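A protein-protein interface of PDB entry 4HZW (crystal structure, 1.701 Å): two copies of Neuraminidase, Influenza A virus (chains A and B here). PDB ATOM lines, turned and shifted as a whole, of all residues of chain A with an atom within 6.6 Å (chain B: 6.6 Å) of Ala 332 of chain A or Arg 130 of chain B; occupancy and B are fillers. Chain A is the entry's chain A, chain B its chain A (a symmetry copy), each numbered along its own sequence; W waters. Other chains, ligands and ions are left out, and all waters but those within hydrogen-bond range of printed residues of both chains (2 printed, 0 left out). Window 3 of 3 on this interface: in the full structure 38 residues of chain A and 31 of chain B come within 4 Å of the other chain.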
ATOM      1  N   LEU A   8     -10.595  -1.710 -32.566  1.00  0.00           N
ATOM      2  CA  LEU A   8     -11.082  -1.053 -31.353  1.00  0.00           C
ATOM      3  C   LEU A   8     -10.877  -1.911 -30.109  1.00  0.00           C
ATOM      4  O   LEU A   8     -10.772  -3.132 -30.200  1.00  0.00           O
ATOM      5  CB  LEU A   8     -12.570  -0.727 -31.496  1.00  0.00           C
ATOM      6  CG  LEU A   8     -12.979   0.071 -32.732  1.00  0.00           C
ATOM      7  CD1 LEU A   8     -14.498   0.141 -32.819  1.00  0.00           C
ATOM      8  CD2 LEU A   8     -12.382   1.460 -32.693  1.00  0.00           C
ATOM      9  N   CYS A  11     -15.401  -3.156 -25.077  1.00  0.00           N
ATOM     10  CA  CYS A  11     -16.169  -2.293 -24.178  1.00  0.00           C
ATOM     11  C   CYS A  11     -16.062  -2.799 -22.743  1.00  0.00           C
ATOM     12  O   CYS A  11     -15.846  -3.983 -22.517  1.00  0.00           O
ATOM     13  CB  CYS A  11     -17.646  -2.253 -24.588  1.00  0.00           C
ATOM     14  SG  CYS A  11     -17.970  -1.618 -26.253  1.00  0.00           S
ATOM     15  N   PHE A  19     -30.200 -11.984 -25.167  1.00  0.00           N
ATOM     16  CA  PHE A  19     -30.277 -11.185 -26.386  1.00  0.00           C
ATOM     17  C   PHE A  19     -31.341 -11.782 -27.318  1.00  0.00           C
ATOM     18  O   PHE A  19     -32.515 -11.368 -27.289  1.00  0.00           O
ATOM     19  CB  PHE A  19     -28.878 -11.180 -27.027  1.00  0.00           C
ATOM     20  CG  PHE A  19     -28.685 -10.183 -28.147  1.00  0.00           C
ATOM     21  CD1 PHE A  19     -29.492  -9.067 -28.278  1.00  0.00           C
ATOM     22  CD2 PHE A  19     -27.648 -10.360 -29.056  1.00  0.00           C
ATOM     23  CE1 PHE A  19     -29.284  -8.158 -29.315  1.00  0.00           C
ATOM     24  CE2 PHE A  19     -27.434  -9.457 -30.087  1.00  0.00           C
ATOM     25  CZ  PHE A  19     -28.256  -8.352 -30.210  1.00  0.00           C
ATOM     26  N   VAL A 330     -19.965  -6.880 -31.452  1.00  0.00           N
ATOM     27  CA  VAL A 330     -20.846  -5.920 -32.098  1.00  0.00           C
ATOM     28  C   VAL A 330     -20.238  -4.543 -31.887  1.00  0.00           C
ATOM     29  O   VAL A 330     -19.842  -4.192 -30.775  1.00  0.00           O
ATOM     30  CB  VAL A 330     -22.266  -5.960 -31.512  1.00  0.00           C
ATOM     31  CG1 VAL A 330     -23.180  -5.044 -32.300  1.00  0.00           C
ATOM     32  CG2 VAL A 330     -22.824  -7.386 -31.534  1.00  0.00           C
ATOM     33  N   LYS A 331     -20.128  -3.771 -32.959  1.00  0.00           N
ATOM     34  CA  LYS A 331     -19.483  -2.470 -32.849  1.00  0.00           C
ATOM     35  C   LYS A 331     -20.348  -1.493 -32.070  1.00  0.00           C
ATOM     36  O   LYS A 331     -21.519  -1.289 -32.390  1.00  0.00           O
ATOM     37  CB  LYS A 331     -19.154  -1.886 -34.223  1.00  0.00           C
ATOM     38  CG  LYS A 331     -18.327  -0.610 -34.120  1.00  0.00           C
ATOM     39  CD  LYS A 331     -18.176   0.100 -35.453  1.00  0.00           C
ATOM     40  CE  LYS A 331     -17.499   1.449 -35.262  1.00  0.00           C
ATOM     41  NZ  LYS A 331     -17.641   2.319 -36.463  1.00  0.00           N
ATOM     42  N   ALA A 332     -19.767  -0.906 -31.032  1.00  0.00           N
ATOM     43  CA  ALA A 332     -20.420   0.168 -30.305  1.00  0.00           C
ATOM     44  C   ALA A 332     -19.864   1.477 -30.852  1.00  0.00           C
ATOM     45  O   ALA A 332     -19.484   1.549 -32.019  1.00  0.00           O
ATOM     46  CB  ALA A 332     -20.161   0.036 -28.824  1.00  0.00           C
ATOM     47  N   LYS A 333     -19.811   2.515 -30.029  1.00  0.00           N
ATOM     48  CA  LYS A 333     -19.265   3.775 -30.509  1.00  0.00           C
ATOM     49  C   LYS A 333     -17.794   3.601 -30.876  1.00  0.00           C
ATOM     50  O   LYS A 333     -17.441   3.495 -32.053  1.00  0.00           O
ATOM     51  CB  LYS A 333     -19.437   4.879 -29.465  1.00  0.00           C
ATOM     52  CG  LYS A 333     -20.882   5.310 -29.271  1.00  0.00           C
ATOM     53  CD  LYS A 333     -21.499   5.736 -30.595  1.00  0.00           C
ATOM     54  CE  LYS A 333     -22.948   6.167 -30.424  1.00  0.00           C
ATOM     55  NZ  LYS A 333     -23.561   6.574 -31.720  1.00  0.00           N
ATOM     56  N   ASP A 334     -16.944   3.552 -29.862  1.00  0.00           N
ATOM     57  CA  ASP A 334     -15.508   3.439 -30.084  1.00  0.00           C
ATOM     58  C   ASP A 334     -14.943   2.199 -29.411  1.00  0.00           C
ATOM     59  O   ASP A 334     -13.770   2.160 -29.041  1.00  0.00           O
ATOM     60  CB  ASP A 334     -14.796   4.695 -29.584  1.00  0.00           C
ATOM     61  CG  ASP A 334     -15.510   5.333 -28.412  1.00  0.00           C
ATOM     62  OD1 ASP A 334     -15.552   6.581 -28.348  1.00  0.00           O
ATOM     63  OD2 ASP A 334     -16.043   4.586 -27.564  1.00  0.00           O
ATOM     64  N   CYS A 335     -15.784   1.182 -29.263  1.00  0.00           N
ATOM     65  CA  CYS A 335     -15.345  -0.093 -28.710  1.00  0.00           C
ATOM     66  C   CYS A 335     -16.193  -1.229 -29.269  1.00  0.00           C
ATOM     67  O   CYS A 335     -17.239  -0.987 -29.865  1.00  0.00           O
ATOM     68  CB  CYS A 335     -15.395  -0.081 -27.176  1.00  0.00           C
ATOM     69  SG  CYS A 335     -17.042   0.192 -26.443  1.00  0.00           S
ATOM     70  N   PHE A 336     -15.728  -2.461 -29.087  1.00  0.00           N
ATOM     71  CA  PHE A 336     -16.502  -3.633 -29.484  1.00  0.00           C
ATOM     72  C   PHE A 336     -17.171  -4.246 -28.266  1.00  0.00           C
ATOM     73  O   PHE A 336     -16.527  -4.468 -27.240  1.00  0.00           O
ATOM     74  CB  PHE A 336     -15.601  -4.683 -30.132  1.00  0.00           C
ATOM     75  CG  PHE A 336     -15.167  -4.334 -31.522  1.00  0.00           C
ATOM     76  CD1 PHE A 336     -16.106  -4.172 -32.529  1.00  0.00           C
ATOM     77  CD2 PHE A 336     -13.826  -4.188 -31.830  1.00  0.00           C
ATOM     78  CE1 PHE A 336     -15.713  -3.863 -33.822  1.00  0.00           C
ATOM     79  CE2 PHE A 336     -13.424  -3.872 -33.125  1.00  0.00           C
ATOM     80  CZ  PHE A 336     -14.369  -3.708 -34.118  1.00  0.00           C
ATOM     81  N   GLN A 337     -18.460  -4.545 -28.386  1.00  0.00           N
ATOM     82  CA  GLN A 337     -19.192  -5.188 -27.305  1.00  0.00           C
ATOM     83  C   GLN A 337     -19.025  -6.707 -27.376  1.00  0.00           C
ATOM     84  O   GLN A 337     -19.238  -7.308 -28.428  1.00  0.00           O
ATOM     85  CB  GLN A 337     -20.671  -4.817 -27.406  1.00  0.00           C
ATOM     86  CG  GLN A 337     -21.569  -5.576 -26.463  1.00  0.00           C
ATOM     87  CD  GLN A 337     -23.022  -5.205 -26.669  1.00  0.00           C
ATOM     88  OE1 GLN A 337     -23.443  -4.921 -27.789  1.00  0.00           O
ATOM     89  NE2 GLN A 337     -23.795  -5.194 -25.591  1.00  0.00           N
ATOM     90  N   ILE B 125     -32.295  -3.082 -23.357  1.00  0.00           N
ATOM     91  CA  ILE B 125     -32.567  -2.006 -24.295  1.00  0.00           C
ATOM     92  C   ILE B 125     -31.807  -2.293 -25.586  1.00  0.00           C
ATOM     93  O   ILE B 125     -30.583  -2.458 -25.570  1.00  0.00           O
ATOM     94  CB  ILE B 125     -32.133  -0.616 -23.741  1.00  0.00           C
ATOM     95  CG1 ILE B 125     -32.733  -0.351 -22.354  1.00  0.00           C
ATOM     96  CG2 ILE B 125     -32.512   0.493 -24.724  1.00  0.00           C
ATOM     97  CD1 ILE B 125     -34.234  -0.512 -22.286  1.00  0.00           C
ATOM     98  N   ILE B 126     -32.539  -2.373 -26.691  1.00  0.00           N
ATOM     99  CA  ILE B 126     -31.951  -2.628 -28.005  1.00  0.00           C
ATOM    100  C   ILE B 126     -32.133  -1.373 -28.842  1.00  0.00           C
ATOM    101  O   ILE B 126     -33.218  -0.789 -28.862  1.00  0.00           O
ATOM    102  CB  ILE B 126     -32.660  -3.786 -28.744  1.00  0.00           C
ATOM    103  CG1 ILE B 126     -32.895  -4.985 -27.819  1.00  0.00           C
ATOM    104  CG2 ILE B 126     -31.879  -4.178 -30.008  1.00  0.00           C
ATOM    105  CD1 ILE B 126     -31.635  -5.582 -27.228  1.00  0.00           C
ATOM    106  N   TYR B 127     -31.070  -0.954 -29.518  1.00  0.00           N
ATOM    107  CA  TYR B 127     -31.129   0.225 -30.371  1.00  0.00           C
ATOM    108  C   TYR B 127     -30.352  -0.046 -31.647  1.00  0.00           C
ATOM    109  O   TYR B 127     -29.154  -0.333 -31.602  1.00  0.00           O
ATOM    110  CB  TYR B 127     -30.560   1.456 -29.657  1.00  0.00           C
ATOM    111  CG  TYR B 127     -30.715   2.721 -30.472  1.00  0.00           C
ATOM    112  CD1 TYR B 127     -31.939   3.379 -30.543  1.00  0.00           C
ATOM    113  CD2 TYR B 127     -29.647   3.242 -31.191  1.00  0.00           C
ATOM    114  CE1 TYR B 127     -32.093   4.528 -31.304  1.00  0.00           C
ATOM    115  CE2 TYR B 127     -29.789   4.396 -31.950  1.00  0.00           C
ATOM    116  CZ  TYR B 127     -31.015   5.032 -32.006  1.00  0.00           C
ATOM    117  OH  TYR B 127     -31.162   6.176 -32.760  1.00  0.00           O
ATOM    118  N   GLY B 128     -31.039   0.034 -32.784  1.00  0.00           N
ATOM    119  CA  GLY B 128     -30.407  -0.277 -34.058  1.00  0.00           C
ATOM    120  C   GLY B 128     -29.843  -1.689 -34.099  1.00  0.00           C
ATOM    121  O   GLY B 128     -28.824  -1.940 -34.749  1.00  0.00           O
ATOM    122  N   GLY B 129     -30.498  -2.609 -33.392  1.00  0.00           N
ATOM    123  CA  GLY B 129     -30.113  -4.012 -33.416  1.00  0.00           C
ATOM    124  C   GLY B 129     -29.079  -4.403 -32.373  1.00  0.00           C
ATOM    125  O   GLY B 129     -28.770  -5.581 -32.208  1.00  0.00           O
ATOM    126  N   ARG B 130     -28.548  -3.417 -31.663  1.00  0.00           N
ATOM    127  CA  ARG B 130     -27.514  -3.677 -30.666  1.00  0.00           C
ATOM    128  C   ARG B 130     -28.054  -3.494 -29.256  1.00  0.00           C
ATOM    129  O   ARG B 130     -28.823  -2.575 -28.997  1.00  0.00           O
ATOM    130  CB  ARG B 130     -26.324  -2.741 -30.869  1.00  0.00           C
ATOM    131  CG  ARG B 130     -25.146  -3.087 -29.977  1.00  0.00           C
ATOM    132  CD  ARG B 130     -23.916  -2.270 -30.334  1.00  0.00           C
ATOM    133  NE  ARG B 130     -23.666  -1.197 -29.378  1.00  0.00           N
ATOM    134  CZ  ARG B 130     -24.039   0.067 -29.545  1.00  0.00           C
ATOM    135  NH1 ARG B 130     -24.695   0.436 -30.638  1.00  0.00           N
ATOM    136  NH2 ARG B 130     -23.758   0.964 -28.609  1.00  0.00           N
ATOM    137  N   MET B 131     -27.643  -4.369 -28.344  1.00  0.00           N
ATOM    138  CA  MET B 131     -28.031  -4.212 -26.949  1.00  0.00           C
ATOM    139  C   MET B 131     -27.159  -3.134 -26.321  1.00  0.00           C
ATOM    140  O   MET B 131     -25.939  -3.287 -26.204  1.00  0.00           O
ATOM    141  CB  MET B 131     -27.894  -5.513 -26.168  1.00  0.00           C
ATOM    142  CG  MET B 131     -28.431  -5.381 -24.745  1.00  0.00           C
ATOM    143  SD  MET B 131     -28.069  -6.832 -23.761  1.00  0.00           S
ATOM    144  CE  MET B 131     -28.909  -8.093 -24.718  1.00  0.00           C
ATOM    145  N   THR B 132     -27.793  -2.044 -25.918  1.00  0.00           N
ATOM    146  CA  THR B 132     -27.074  -0.834 -25.537  1.00  0.00           C
ATOM    147  C   THR B 132     -27.168  -0.518 -24.043  1.00  0.00           C
ATOM    148  O   THR B 132     -26.323   0.197 -23.503  1.00  0.00           O
ATOM    149  CB  THR B 132     -27.604   0.379 -26.315  1.00  0.00           C
ATOM    150  OG1 THR B 132     -29.025   0.452 -26.166  1.00  0.00           O
ATOM    151  CG2 THR B 132     -27.277   0.255 -27.800  1.00  0.00           C
ATOM    152  N   ASP B 133     -28.198  -1.027 -23.376  1.00  0.00           N
ATOM    153  CA  ASP B 133     -28.386  -0.720 -21.956  1.00  0.00           C
ATOM    154  C   ASP B 133     -29.332  -1.736 -21.335  1.00  0.00           C
ATOM    155  O   ASP B 133     -29.822  -2.633 -22.020  1.00  0.00           O
ATOM    156  CB  ASP B 133     -28.920   0.707 -21.773  1.00  0.00           C
ATOM    157  CG  ASP B 133     -28.336   1.411 -20.549  1.00  0.00           C
ATOM    158  OD1 ASP B 133     -27.982   0.731 -19.562  1.00  0.00           O
ATOM    159  OD2 ASP B 133     -28.230   2.659 -20.578  1.00  0.00           O
ATOM    160  N   GLU B 179     -30.682   7.209 -28.122  1.00  0.00           N
ATOM    161  CA  GLU B 179     -29.801   6.332 -28.881  1.00  0.00           C
ATOM    162  C   GLU B 179     -29.438   5.083 -28.083  1.00  0.00           C
ATOM    163  O   GLU B 179     -28.316   4.583 -28.160  1.00  0.00           O
ATOM    164  CB  GLU B 179     -28.551   7.084 -29.350  1.00  0.00           C
ATOM    165  CG  GLU B 179     -28.876   8.236 -30.296  1.00  0.00           C
ATOM    166  CD  GLU B 179     -27.669   9.109 -30.603  1.00  0.00           C
ATOM    167  OE1 GLU B 179     -26.535   8.717 -30.253  1.00  0.00           O
ATOM    168  OE2 GLU B 179     -27.858  10.191 -31.198  1.00  0.00           O
ATOM    169  N   GLY B 180     -30.400   4.588 -27.311  1.00  0.00           N
ATOM    170  CA  GLY B 180     -30.248   3.323 -26.618  1.00  0.00           C
ATOM    171  C   GLY B 180     -29.651   3.435 -25.228  1.00  0.00           C
ATOM    172  O   GLY B 180     -29.565   2.441 -24.513  1.00  0.00           O
ATOM    173  N   LYS B 181     -29.252   4.644 -24.843  1.00  0.00           N
ATOM    174  CA  LYS B 181     -28.656   4.875 -23.526  1.00  0.00           C
ATOM    175  C   LYS B 181     -29.652   5.513 -22.575  1.00  0.00           C
ATOM    176  O   LYS B 181     -30.260   6.530 -22.890  1.00  0.00           O
ATOM    177  CB  LYS B 181     -27.425   5.767 -23.641  1.00  0.00           C
ATOM    178  CG  LYS B 181     -26.302   5.157 -24.469  1.00  0.00           C
ATOM    179  CD  LYS B 181     -25.798   3.852 -23.859  1.00  0.00           C
ATOM    180  CE  LYS B 181     -24.782   3.175 -24.768  1.00  0.00           C
ATOM    181  NZ  LYS B 181     -24.053   2.068 -24.081  1.00  0.00           N
HETATM  182  O   HOH W   1     -23.527  -1.773 -26.982  1.00  0.00           O
HETATM  183  O   HOH W   2     -25.613  -6.229 -28.978  1.00  0.00           O
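NZ of Lys 333 of chain A is in salt-bridge range of OE1 of Glu 179 of chain B, 3.9 Å away. O of Met 131 of chain B lies within hydrogen-bond range of NE2 of Gln 337 of chain A.
SG of Cys 11 of chain A sits at hydrogen-bond distance from N of Gln 337 of chain A, at 3.7 Å. The backbone carbonyl oxygen (O) of Val 330 of chain A is in hydrogen-bond range of the backbone NH (N) of Gln 337 of chain A (2.8 Å). The side-chain sulfur (SG) of Cys 11 of chain A is disulfide-bonded to the side-chain sulfur (SG) of Cys 335 of chain A.
O of Gly 129 of chain B touches CZ of Phe 19 of chain A, at 3.5 Å. Phe 19 of chain A touches Met 131 of chain B. Val 330 of chain A touches Arg 130 of chain B. O of Lys 331 of chain A touches CD of Arg 130 of chain B, 3.3 Å away. Ala 332 of chain A touches Arg 130 of chain B (CA to NE, 3.6 Å). Arg 130 of chain B touches Gln 337 of chain A.
Of chain B, only Arg 130 comes within 4 Å of Ala 332 of chain A. Of chain A, only Val 330 (3.5 Å), Lys 331 (3.3 Å), Ala 332 (3.6 Å) and Gln 337 (3.3 Å) come within 4 Å of Arg 130 of chain B. Of the printed residues of chain A, Met 131 of chain B touches Phe 19 and Gln 337. Of the printed residues of chain A, Glu 179 of chain B touches Lys 333. Of the printed residues of chain A, Gly 129 of chain B touches Phe 19. Of the printed residues of chain B, Phe 19 of chain A touches Gly 129 and Met 131. The nearest residue of chain B that does not touch Ala 332 of chain A is Lys 181 of chain B (6.5 Å).
Hydrophobic or aromatic side chains of chain B that line the printed part of chain A: Met 131. Of the 11 printed residues of chain A, 6 touch a printed residue of chain B. Among the printed residues, 8 pairs touch across the chains.
No position is printed for both chains. Of the 8 pairs that touch across the chains among the printed residues, none has its exchanged pair printed and touching as well.
Water W1 lies within hydrogen-bond range of NE of Arg 130 of chain B, O of Met 131 of chain B and OE1 of Gln 337 of chain A. Water W2 bridges OE1 of Gln 337 of chain A and N of Met 131 of chain B.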
